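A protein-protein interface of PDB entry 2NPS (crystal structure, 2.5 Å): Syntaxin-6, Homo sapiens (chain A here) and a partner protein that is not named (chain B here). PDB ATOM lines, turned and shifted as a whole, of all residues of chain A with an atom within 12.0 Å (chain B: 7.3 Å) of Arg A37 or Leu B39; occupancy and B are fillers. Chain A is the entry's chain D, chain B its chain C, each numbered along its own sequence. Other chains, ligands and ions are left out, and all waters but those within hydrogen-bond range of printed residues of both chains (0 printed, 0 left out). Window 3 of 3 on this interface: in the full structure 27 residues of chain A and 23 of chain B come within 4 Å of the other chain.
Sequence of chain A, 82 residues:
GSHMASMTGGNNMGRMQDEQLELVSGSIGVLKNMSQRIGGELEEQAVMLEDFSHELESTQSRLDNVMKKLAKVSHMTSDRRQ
The side-chain sulfur (SD) of Met A34 sits at hydrogen-bond distance from the backbone NH (N) of Gln B36 (3.6 Å). The side-chain amide nitrogen of Gln A45 sits at hydrogen-bond distance from the backbone carbonyl oxygen of Leu B42, 3.0 Å away.
The side-chain amide oxygen (OD1) of Asn A33 lies within hydrogen-bond range of the guanidinium group (NH2) of Arg A37. The side-chain carboxylate of Glu A41 is in hydrogen-bond range of the side-chain amide nitrogen of Gln A45, at 3.0 Å.
C of Gly B35 touches SD of Met A34 (3.9 Å). CD1 of Leu B39 touches NH1 of Arg A37, at 3.2 Å. Ile A38 touches Leu B39. Leu A42 touches Leu B42 (CD2 to CD2, 3.9 Å).
Of the printed residues of chain B, Met A34 touches Gly B35 and Gln B36. Of the printed residues of chain B, Arg A37 touches Leu B39. Printed residues of chain B within 4 Å of Gln A45: Leu B42. Gly B35 touches just one residue of chain A: Met A34 (3.9 Å). Of chain A, only Met A34 comes within 4 Å of Gln B36. No residue of chain A comes within 4 Å of Glu B37. Met B38 touches none of the printed residues of chain A. Glu B40 touches none of the printed residues of chain A. No residue of chain A comes within 4 Å of Asn B41. No residue of chain A comes within 4 Å of Ser B43. The nearest printed residue of chain B that does not touch Leu A42 is Met B38 (7.1 Å).
Of the 22 printed residues of chain A, 5 touch a printed residue of chain B. Printed residues of chain A that touch a printed residue of chain B: Met A34, Arg A37, Ile A38, Leu A42 and Gln A45. Among the printed residues, 6 pairs touch across the chains.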
ATOM      1  N   GLY A  26      19.348 -30.952  30.922  1.00  0.00           N
ATOM      2  CA  GLY A  26      18.087 -31.628  30.707  1.00  0.00           C
ATOM      3  C   GLY A  26      17.006 -30.574  30.788  1.00  0.00           C
ATOM      4  O   GLY A  26      16.224 -30.385  29.856  1.00  0.00           O
ATOM      5  N   SER A  27      16.982 -29.875  31.916  1.00  0.00           N
ATOM      6  CA  SER A  27      15.997 -28.832  32.155  1.00  0.00           C
ATOM      7  C   SER A  27      15.870 -27.893  30.973  1.00  0.00           C
ATOM      8  O   SER A  27      14.765 -27.598  30.524  1.00  0.00           O
ATOM      9  CB  SER A  27      16.369 -28.023  33.398  1.00  0.00           C
ATOM     10  OG  SER A  27      15.502 -26.903  33.550  1.00  0.00           O
ATOM     11  N   ILE A  28      17.007 -27.423  30.475  1.00  0.00           N
ATOM     12  CA  ILE A  28      17.013 -26.506  29.350  1.00  0.00           C
ATOM     13  C   ILE A  28      16.468 -27.155  28.090  1.00  0.00           C
ATOM     14  O   ILE A  28      15.703 -26.540  27.350  1.00  0.00           O
ATOM     15  CB  ILE A  28      18.415 -25.990  29.051  1.00  0.00           C
ATOM     16  CG1 ILE A  28      18.387 -25.145  27.783  1.00  0.00           C
ATOM     17  CG2 ILE A  28      19.355 -27.143  28.849  1.00  0.00           C
ATOM     18  N   GLY A  29      16.876 -28.396  27.844  1.00  0.00           N
ATOM     19  CA  GLY A  29      16.412 -29.107  26.669  1.00  0.00           C
ATOM     20  C   GLY A  29      14.912 -28.968  26.534  1.00  0.00           C
ATOM     21  O   GLY A  29      14.398 -28.655  25.461  1.00  0.00           O
ATOM     22  N   VAL A  30      14.212 -29.203  27.642  1.00  0.00           N
ATOM     23  CA  VAL A  30      12.755 -29.099  27.682  1.00  0.00           C
ATOM     24  C   VAL A  30      12.331 -27.686  27.277  1.00  0.00           C
ATOM     25  O   VAL A  30      11.418 -27.504  26.464  1.00  0.00           O
ATOM     26  CB  VAL A  30      12.212 -29.391  29.096  1.00  0.00           C
ATOM     27  CG1 VAL A  30      10.712 -29.128  29.152  1.00  0.00           C
ATOM     28  CG2 VAL A  30      12.506 -30.829  29.466  1.00  0.00           C
ATOM     29  N   LEU A  31      12.996 -26.687  27.850  1.00  0.00           N
ATOM     30  CA  LEU A  31      12.701 -25.297  27.531  1.00  0.00           C
ATOM     31  C   LEU A  31      12.876 -25.148  26.034  1.00  0.00           C
ATOM     32  O   LEU A  31      12.114 -24.447  25.374  1.00  0.00           O
ATOM     33  CB  LEU A  31      13.669 -24.357  28.254  1.00  0.00           C
ATOM     34  CG  LEU A  31      13.579 -24.330  29.776  1.00  0.00           C
ATOM     35  N   LYS A  32      13.893 -25.820  25.506  1.00  0.00           N
ATOM     36  CA  LYS A  32      14.173 -25.795  24.077  1.00  0.00           C
ATOM     37  C   LYS A  32      13.042 -26.503  23.350  1.00  0.00           C
ATOM     38  O   LYS A  32      12.817 -26.278  22.167  1.00  0.00           O
ATOM     39  CB  LYS A  32      15.491 -26.504  23.775  1.00  0.00           C
ATOM     40  CG  LYS A  32      15.757 -26.688  22.294  1.00  0.00           C
ATOM     41  N   ASN A  33      12.340 -27.374  24.068  1.00  0.00           N
ATOM     42  CA  ASN A  33      11.222 -28.101  23.485  1.00  0.00           C
ATOM     43  C   ASN A  33       9.995 -27.228  23.531  1.00  0.00           C
ATOM     44  O   ASN A  33       9.318 -27.041  22.524  1.00  0.00           O
ATOM     45  CB  ASN A  33      10.927 -29.388  24.258  1.00  0.00           C
ATOM     46  CG  ASN A  33       9.654 -30.069  23.785  1.00  0.00           C
ATOM     47  OD1 ASN A  33       8.612 -30.015  24.452  1.00  0.00           O
ATOM     48  ND2 ASN A  33       9.730 -30.708  22.618  1.00  0.00           N
ATOM     49  N   MET A  34       9.711 -26.702  24.715  1.00  0.00           N
ATOM     50  CA  MET A  34       8.547 -25.860  24.915  1.00  0.00           C
ATOM     51  C   MET A  34       8.582 -24.617  24.057  1.00  0.00           C
ATOM     52  O   MET A  34       7.554 -24.185  23.562  1.00  0.00           O
ATOM     53  CB  MET A  34       8.423 -25.455  26.383  1.00  0.00           C
ATOM     54  CG  MET A  34       7.953 -26.555  27.313  1.00  0.00           C
ATOM     55  SD  MET A  34       7.822 -25.969  29.033  1.00  0.00           S
ATOM     56  CE  MET A  34       7.488 -27.492  29.870  1.00  0.00           C
ATOM     57  N   SER A  35       9.759 -24.036  23.876  1.00  0.00           N
ATOM     58  CA  SER A  35       9.839 -22.833  23.072  1.00  0.00           C
ATOM     59  C   SER A  35       9.419 -23.106  21.633  1.00  0.00           C
ATOM     60  O   SER A  35       8.710 -22.310  21.027  1.00  0.00           O
ATOM     61  CB  SER A  35      11.252 -22.238  23.111  1.00  0.00           C
ATOM     62  OG  SER A  35      12.189 -23.072  22.466  1.00  0.00           O
ATOM     63  N   GLN A  36       9.826 -24.245  21.087  1.00  0.00           N
ATOM     64  CA  GLN A  36       9.476 -24.580  19.708  1.00  0.00           C
ATOM     65  C   GLN A  36       8.002 -24.898  19.489  1.00  0.00           C
ATOM     66  O   GLN A  36       7.409 -24.458  18.511  1.00  0.00           O
ATOM     67  CB  GLN A  36      10.324 -25.746  19.215  1.00  0.00           C
ATOM     68  CG  GLN A  36      11.804 -25.524  19.369  1.00  0.00           C
ATOM     69  CD  GLN A  36      12.606 -26.584  18.669  1.00  0.00           C
ATOM     70  OE1 GLN A  36      12.631 -26.639  17.436  1.00  0.00           O
ATOM     71  NE2 GLN A  36      13.264 -27.447  19.445  1.00  0.00           N
ATOM     72  N   ARG A  37       7.410 -25.675  20.384  1.00  0.00           N
ATOM     73  CA  ARG A  37       5.997 -26.001  20.260  1.00  0.00           C
ATOM     74  C   ARG A  37       5.178 -24.704  20.314  1.00  0.00           C
ATOM     75  O   ARG A  37       4.102 -24.610  19.727  1.00  0.00           O
ATOM     76  CB  ARG A  37       5.576 -26.943  21.387  1.00  0.00           C
ATOM     77  CG  ARG A  37       6.191 -28.344  21.294  1.00  0.00           C
ATOM     78  CD  ARG A  37       6.220 -29.043  22.654  1.00  0.00           C
ATOM     79  NE  ARG A  37       4.911 -29.056  23.303  1.00  0.00           N
ATOM     80  CZ  ARG A  37       4.730 -29.227  24.610  1.00  0.00           C
ATOM     81  NH1 ARG A  37       3.507 -29.230  25.119  1.00  0.00           N
ATOM     82  NH2 ARG A  37       5.774 -29.388  25.420  1.00  0.00           N
ATOM     83  N   ILE A  38       5.715 -23.714  21.027  1.00  0.00           N
ATOM     84  CA  ILE A  38       5.109 -22.398  21.189  1.00  0.00           C
ATOM     85  C   ILE A  38       5.194 -21.657  19.874  1.00  0.00           C
ATOM     86  O   ILE A  38       4.236 -21.018  19.447  1.00  0.00           O
ATOM     87  CB  ILE A  38       5.862 -21.574  22.254  1.00  0.00           C
ATOM     88  CG1 ILE A  38       5.626 -22.179  23.641  1.00  0.00           C
ATOM     89  CG2 ILE A  38       5.429 -20.116  22.193  1.00  0.00           C
ATOM     90  CD1 ILE A  38       6.529 -21.610  24.717  1.00  0.00           C
ATOM     91  N   GLY A  39       6.357 -21.733  19.241  1.00  0.00           N
ATOM     92  CA  GLY A  39       6.547 -21.075  17.965  1.00  0.00           C
ATOM     93  C   GLY A  39       5.681 -21.715  16.897  1.00  0.00           C
ATOM     94  O   GLY A  39       5.154 -21.024  16.017  1.00  0.00           O
ATOM     95  N   GLY A  40       5.533 -23.039  16.982  1.00  0.00           N
ATOM     96  CA  GLY A  40       4.720 -23.767  16.025  1.00  0.00           C
ATOM     97  C   GLY A  40       3.262 -23.380  16.153  1.00  0.00           C
ATOM     98  O   GLY A  40       2.589 -23.063  15.161  1.00  0.00           O
ATOM     99  N   GLU A  41       2.778 -23.405  17.390  1.00  0.00           N
ATOM    100  CA  GLU A  41       1.405 -23.035  17.703  1.00  0.00           C
ATOM    101  C   GLU A  41       1.154 -21.569  17.317  1.00  0.00           C
ATOM    102  O   GLU A  41       0.091 -21.217  16.808  1.00  0.00           O
ATOM    103  CB  GLU A  41       1.152 -23.233  19.195  1.00  0.00           C
ATOM    104  CG  GLU A  41      -0.275 -22.953  19.624  1.00  0.00           C
ATOM    105  CD  GLU A  41      -1.271 -23.751  18.816  1.00  0.00           C
ATOM    106  OE1 GLU A  41      -1.200 -25.004  18.825  1.00  0.00           O
ATOM    107  OE2 GLU A  41      -2.130 -23.122  18.166  1.00  0.00           O
ATOM    108  N   LEU A  42       2.134 -20.706  17.557  1.00  0.00           N
ATOM    109  CA  LEU A  42       1.961 -19.306  17.206  1.00  0.00           C
ATOM    110  C   LEU A  42       1.862 -19.149  15.697  1.00  0.00           C
ATOM    111  O   LEU A  42       1.105 -18.324  15.198  1.00  0.00           O
ATOM    112  CB  LEU A  42       3.119 -18.469  17.749  1.00  0.00           C
ATOM    113  CG  LEU A  42       3.099 -18.220  19.258  1.00  0.00           C
ATOM    114  CD1 LEU A  42       4.407 -17.593  19.722  1.00  0.00           C
ATOM    115  CD2 LEU A  42       1.929 -17.322  19.596  1.00  0.00           C
ATOM    116  N   GLU A  43       2.628 -19.947  14.964  1.00  0.00           N
ATOM    117  CA  GLU A  43       2.593 -19.860  13.513  1.00  0.00           C
ATOM    118  C   GLU A  43       1.266 -20.391  12.990  1.00  0.00           C
ATOM    119  O   GLU A  43       0.709 -19.862  12.035  1.00  0.00           O
ATOM    120  CB  GLU A  43       3.763 -20.633  12.912  1.00  0.00           C
ATOM    121  CG  GLU A  43       3.943 -20.386  11.431  1.00  0.00           C
ATOM    122  CD  GLU A  43       3.834 -18.916  11.063  1.00  0.00           C
ATOM    123  N   GLU A  44       0.757 -21.426  13.650  1.00  0.00           N
ATOM    124  CA  GLU A  44      -0.521 -22.038  13.307  1.00  0.00           C
ATOM    125  C   GLU A  44      -1.697 -21.108  13.556  1.00  0.00           C
ATOM    126  O   GLU A  44      -2.684 -21.111  12.814  1.00  0.00           O
ATOM    127  CB  GLU A  44      -0.746 -23.292  14.125  1.00  0.00           C
ATOM    128  CG  GLU A  44      -0.074 -24.508  13.575  1.00  0.00           C
ATOM    129  CD  GLU A  44      -0.622 -25.758  14.209  1.00  0.00           C
ATOM    130  OE1 GLU A  44      -0.178 -26.866  13.837  1.00  0.00           O
ATOM    131  OE2 GLU A  44      -1.507 -25.615  15.085  1.00  0.00           O
ATOM    132  N   GLN A  45      -1.606 -20.328  14.622  1.00  0.00           N
ATOM    133  CA  GLN A  45      -2.660 -19.390  14.938  1.00  0.00           C
ATOM    134  C   GLN A  45      -2.567 -18.199  14.001  1.00  0.00           C
ATOM    135  O   GLN A  45      -3.573 -17.614  13.629  1.00  0.00           O
ATOM    136  CB  GLN A  45      -2.558 -18.974  16.397  1.00  0.00           C
ATOM    137  CG  GLN A  45      -3.120 -20.034  17.322  1.00  0.00           C
ATOM    138  CD  GLN A  45      -3.090 -19.633  18.776  1.00  0.00           C
ATOM    139  OE1 GLN A  45      -3.165 -18.455  19.106  1.00  0.00           O
ATOM    140  NE2 GLN A  45      -3.004 -20.618  19.660  1.00  0.00           N
ATOM    141  N   ALA A  46      -1.355 -17.864  13.584  1.00  0.00           N
ATOM    142  CA  ALA A  46      -1.178 -16.772  12.645  1.00  0.00           C
ATOM    143  C   ALA A  46      -1.997 -17.090  11.391  1.00  0.00           C
ATOM    144  O   ALA A  46      -2.706 -16.243  10.858  1.00  0.00           O
ATOM    145  CB  ALA A  46       0.292 -16.613  12.302  1.00  0.00           C
ATOM    146  N   MET A  48      -4.506 -19.246  11.224  1.00  0.00           N
ATOM    147  CA  MET A  48      -5.882 -19.252  11.689  1.00  0.00           C
ATOM    148  C   MET A  48      -6.463 -17.845  11.872  1.00  0.00           C
ATOM    149  O   MET A  48      -7.654 -17.634  11.675  1.00  0.00           O
ATOM    150  CB  MET A  48      -5.944 -20.032  13.002  1.00  0.00           C
ATOM    151  CG  MET A  48      -7.303 -20.551  13.403  1.00  0.00           C
ATOM    152  SD  MET A  48      -7.239 -21.251  15.069  1.00  0.00           S
ATOM    153  CE  MET A  48      -6.170 -22.625  14.802  1.00  0.00           C
ATOM    154  N   ILE B  34       6.314 -21.873  33.355  1.00  0.00           N
ATOM    155  CA  ILE B  34       5.801 -20.729  32.623  1.00  0.00           C
ATOM    156  C   ILE B  34       5.555 -21.170  31.186  1.00  0.00           C
ATOM    157  O   ILE B  34       4.469 -20.993  30.648  1.00  0.00           O
ATOM    158  CB  ILE B  34       6.798 -19.570  32.617  1.00  0.00           C
ATOM    159  CG1 ILE B  34       7.117 -19.148  34.051  1.00  0.00           C
ATOM    160  CG2 ILE B  34       6.234 -18.420  31.809  1.00  0.00           C
ATOM    161  CD1 ILE B  34       8.039 -17.934  34.143  1.00  0.00           C
ATOM    162  N   GLY B  35       6.575 -21.754  30.572  1.00  0.00           N
ATOM    163  CA  GLY B  35       6.445 -22.229  29.206  1.00  0.00           C
ATOM    164  C   GLY B  35       5.222 -23.110  29.043  1.00  0.00           C
ATOM    165  O   GLY B  35       4.523 -23.024  28.034  1.00  0.00           O
ATOM    166  N   GLN B  36       4.959 -23.956  30.039  1.00  0.00           N
ATOM    167  CA  GLN B  36       3.803 -24.844  29.996  1.00  0.00           C
ATOM    168  C   GLN B  36       2.541 -24.006  30.095  1.00  0.00           C
ATOM    169  O   GLN B  36       1.576 -24.234  29.371  1.00  0.00           O
ATOM    170  CB  GLN B  36       3.821 -25.830  31.163  1.00  0.00           C
ATOM    171  CG  GLN B  36       2.688 -26.853  31.120  1.00  0.00           C
ATOM    172  CD  GLN B  36       2.882 -27.869  30.014  1.00  0.00           C
ATOM    173  OE1 GLN B  36       3.136 -27.507  28.858  1.00  0.00           O
ATOM    174  NE2 GLN B  36       2.767 -29.151  30.358  1.00  0.00           N
ATOM    175  N   GLU B  37       2.555 -23.033  30.994  1.00  0.00           N
ATOM    176  CA  GLU B  37       1.400 -22.180  31.177  1.00  0.00           C
ATOM    177  C   GLU B  37       1.033 -21.500  29.862  1.00  0.00           C
ATOM    178  O   GLU B  37      -0.138 -21.428  29.502  1.00  0.00           O
ATOM    179  CB  GLU B  37       1.678 -21.148  32.264  1.00  0.00           C
ATOM    180  CG  GLU B  37       0.507 -20.972  33.210  1.00  0.00           C
ATOM    181  CD  GLU B  37      -0.753 -20.536  32.481  1.00  0.00           C
ATOM    182  OE1 GLU B  37      -1.870 -20.856  32.956  1.00  0.00           O
ATOM    183  OE2 GLU B  37      -0.622 -19.863  31.432  1.00  0.00           O
ATOM    184  N   MET B  38       2.031 -21.019  29.130  1.00  0.00           N
ATOM    185  CA  MET B  38       1.771 -20.385  27.842  1.00  0.00           C
ATOM    186  C   MET B  38       1.046 -21.355  26.919  1.00  0.00           C
ATOM    187  O   MET B  38       0.080 -20.982  26.259  1.00  0.00           O
ATOM    188  CB  MET B  38       3.073 -19.948  27.176  1.00  0.00           C
ATOM    189  CG  MET B  38       3.604 -18.617  27.645  1.00  0.00           C
ATOM    190  SD  MET B  38       5.114 -18.171  26.769  1.00  0.00           S
ATOM    191  CE  MET B  38       6.317 -18.914  27.828  1.00  0.00           C
ATOM    192  N   LEU B  39       1.512 -22.599  26.879  1.00  0.00           N
ATOM    193  CA  LEU B  39       0.903 -23.617  26.028  1.00  0.00           C
ATOM    194  C   LEU B  39      -0.550 -23.890  26.420  1.00  0.00           C
ATOM    195  O   LEU B  39      -1.398 -24.159  25.577  1.00  0.00           O
ATOM    196  CB  LEU B  39       1.731 -24.902  26.086  1.00  0.00           C
ATOM    197  CG  LEU B  39       3.071 -24.816  25.346  1.00  0.00           C
ATOM    198  CD1 LEU B  39       3.887 -26.085  25.573  1.00  0.00           C
ATOM    199  CD2 LEU B  39       2.821 -24.608  23.841  1.00  0.00           C
ATOM    200  N   GLU B  40      -0.832 -23.817  27.709  1.00  0.00           N
ATOM    201  CA  GLU B  40      -2.187 -24.018  28.184  1.00  0.00           C
ATOM    202  C   GLU B  40      -3.004 -22.804  27.736  1.00  0.00           C
ATOM    203  O   GLU B  40      -4.132 -22.936  27.278  1.00  0.00           O
ATOM    204  CB  GLU B  40      -2.199 -24.101  29.706  1.00  0.00           C
ATOM    205  CG  GLU B  40      -3.548 -23.846  30.326  1.00  0.00           C
ATOM    206  N   ASN B  41      -2.402 -21.625  27.874  1.00  0.00           N
ATOM    207  CA  ASN B  41      -3.005 -20.340  27.521  1.00  0.00           C
ATOM    208  C   ASN B  41      -3.320 -20.241  26.026  1.00  0.00           C
ATOM    209  O   ASN B  41      -4.427 -19.872  25.640  1.00  0.00           O
ATOM    210  CB  ASN B  41      -2.036 -19.228  27.959  1.00  0.00           C
ATOM    211  CG  ASN B  41      -2.597 -17.825  27.792  1.00  0.00           C
ATOM    212  OD1 ASN B  41      -2.510 -17.003  28.709  1.00  0.00           O
ATOM    213  ND2 ASN B  41      -3.141 -17.531  26.614  1.00  0.00           N
ATOM    214  N   LEU B  42      -2.345 -20.584  25.192  1.00  0.00           N
ATOM    215  CA  LEU B  42      -2.509 -20.534  23.740  1.00  0.00           C
ATOM    216  C   LEU B  42      -3.571 -21.493  23.226  1.00  0.00           C
ATOM    217  O   LEU B  42      -4.303 -21.180  22.298  1.00  0.00           O
ATOM    218  CB  LEU B  42      -1.177 -20.827  23.057  1.00  0.00           C
ATOM    219  CG  LEU B  42      -0.127 -19.731  23.223  1.00  0.00           C
ATOM    220  CD1 LEU B  42       1.259 -20.234  22.880  1.00  0.00           C
ATOM    221  CD2 LEU B  42      -0.517 -18.551  22.353  1.00  0.00           C
ATOM    222  N   SER B  43      -3.650 -22.669  23.829  1.00  0.00           N
ATOM    223  CA  SER B  43      -4.644 -23.647  23.434  1.00  0.00           C
ATOM    224  C   SER B  43      -6.019 -23.065  23.712  1.00  0.00           C
ATOM    225  O   SER B  43      -6.940 -23.187  22.911  1.00  0.00           O
ATOM    226  CB  SER B  43      -4.458 -24.935  24.231  1.00  0.00           C
ATOM    227  N   HIS B  44      -6.135 -22.417  24.857  1.00  0.00           N
ATOM    228  CA  HIS B  44      -7.379 -21.811  25.283  1.00  0.00           C
ATOM    229  C   HIS B  44      -7.807 -20.725  24.300  1.00  0.00           C
ATOM    230  O   HIS B  44      -8.975 -20.624  23.924  1.00  0.00           O
ATOM    231  CB  HIS B  44      -7.197 -21.214  26.675  1.00  0.00           C
ATOM    232  CG  HIS B  44      -8.467 -21.114  27.460  1.00  0.00           C
ATOM    233  ND1 HIS B  44      -8.999 -22.183  28.152  1.00  0.00           N
ATOM    234  CD2 HIS B  44      -9.329 -20.082  27.635  1.00  0.00           C
ATOM    235  CE1 HIS B  44     -10.136 -21.815  28.718  1.00  0.00           C
ATOM    236  NE2 HIS B  44     -10.360 -20.545  28.419  1.00  0.00           N
ATOM    237  N   ASP B  45      -6.848 -19.913  23.874  1.00  0.00           N
ATOM    238  CA  ASP B  45      -7.134 -18.841  22.934  1.00  0.00           C
ATOM    239  C   ASP B  45      -7.498 -19.429  21.585  1.00  0.00           C
ATOM    240  O   ASP B  45      -8.474 -19.011  20.965  1.00  0.00           O
ATOM    241  CB  ASP B  45      -5.924 -17.917  22.827  1.00  0.00           C
ATOM    242  CG  ASP B  45      -5.602 -17.242  24.147  1.00  0.00           C
ATOM    243  OD1 ASP B  45      -4.450 -16.791  24.329  1.00  0.00           O
ATOM    244  OD2 ASP B  45      -6.515 -17.159  25.006  1.00  0.00           O
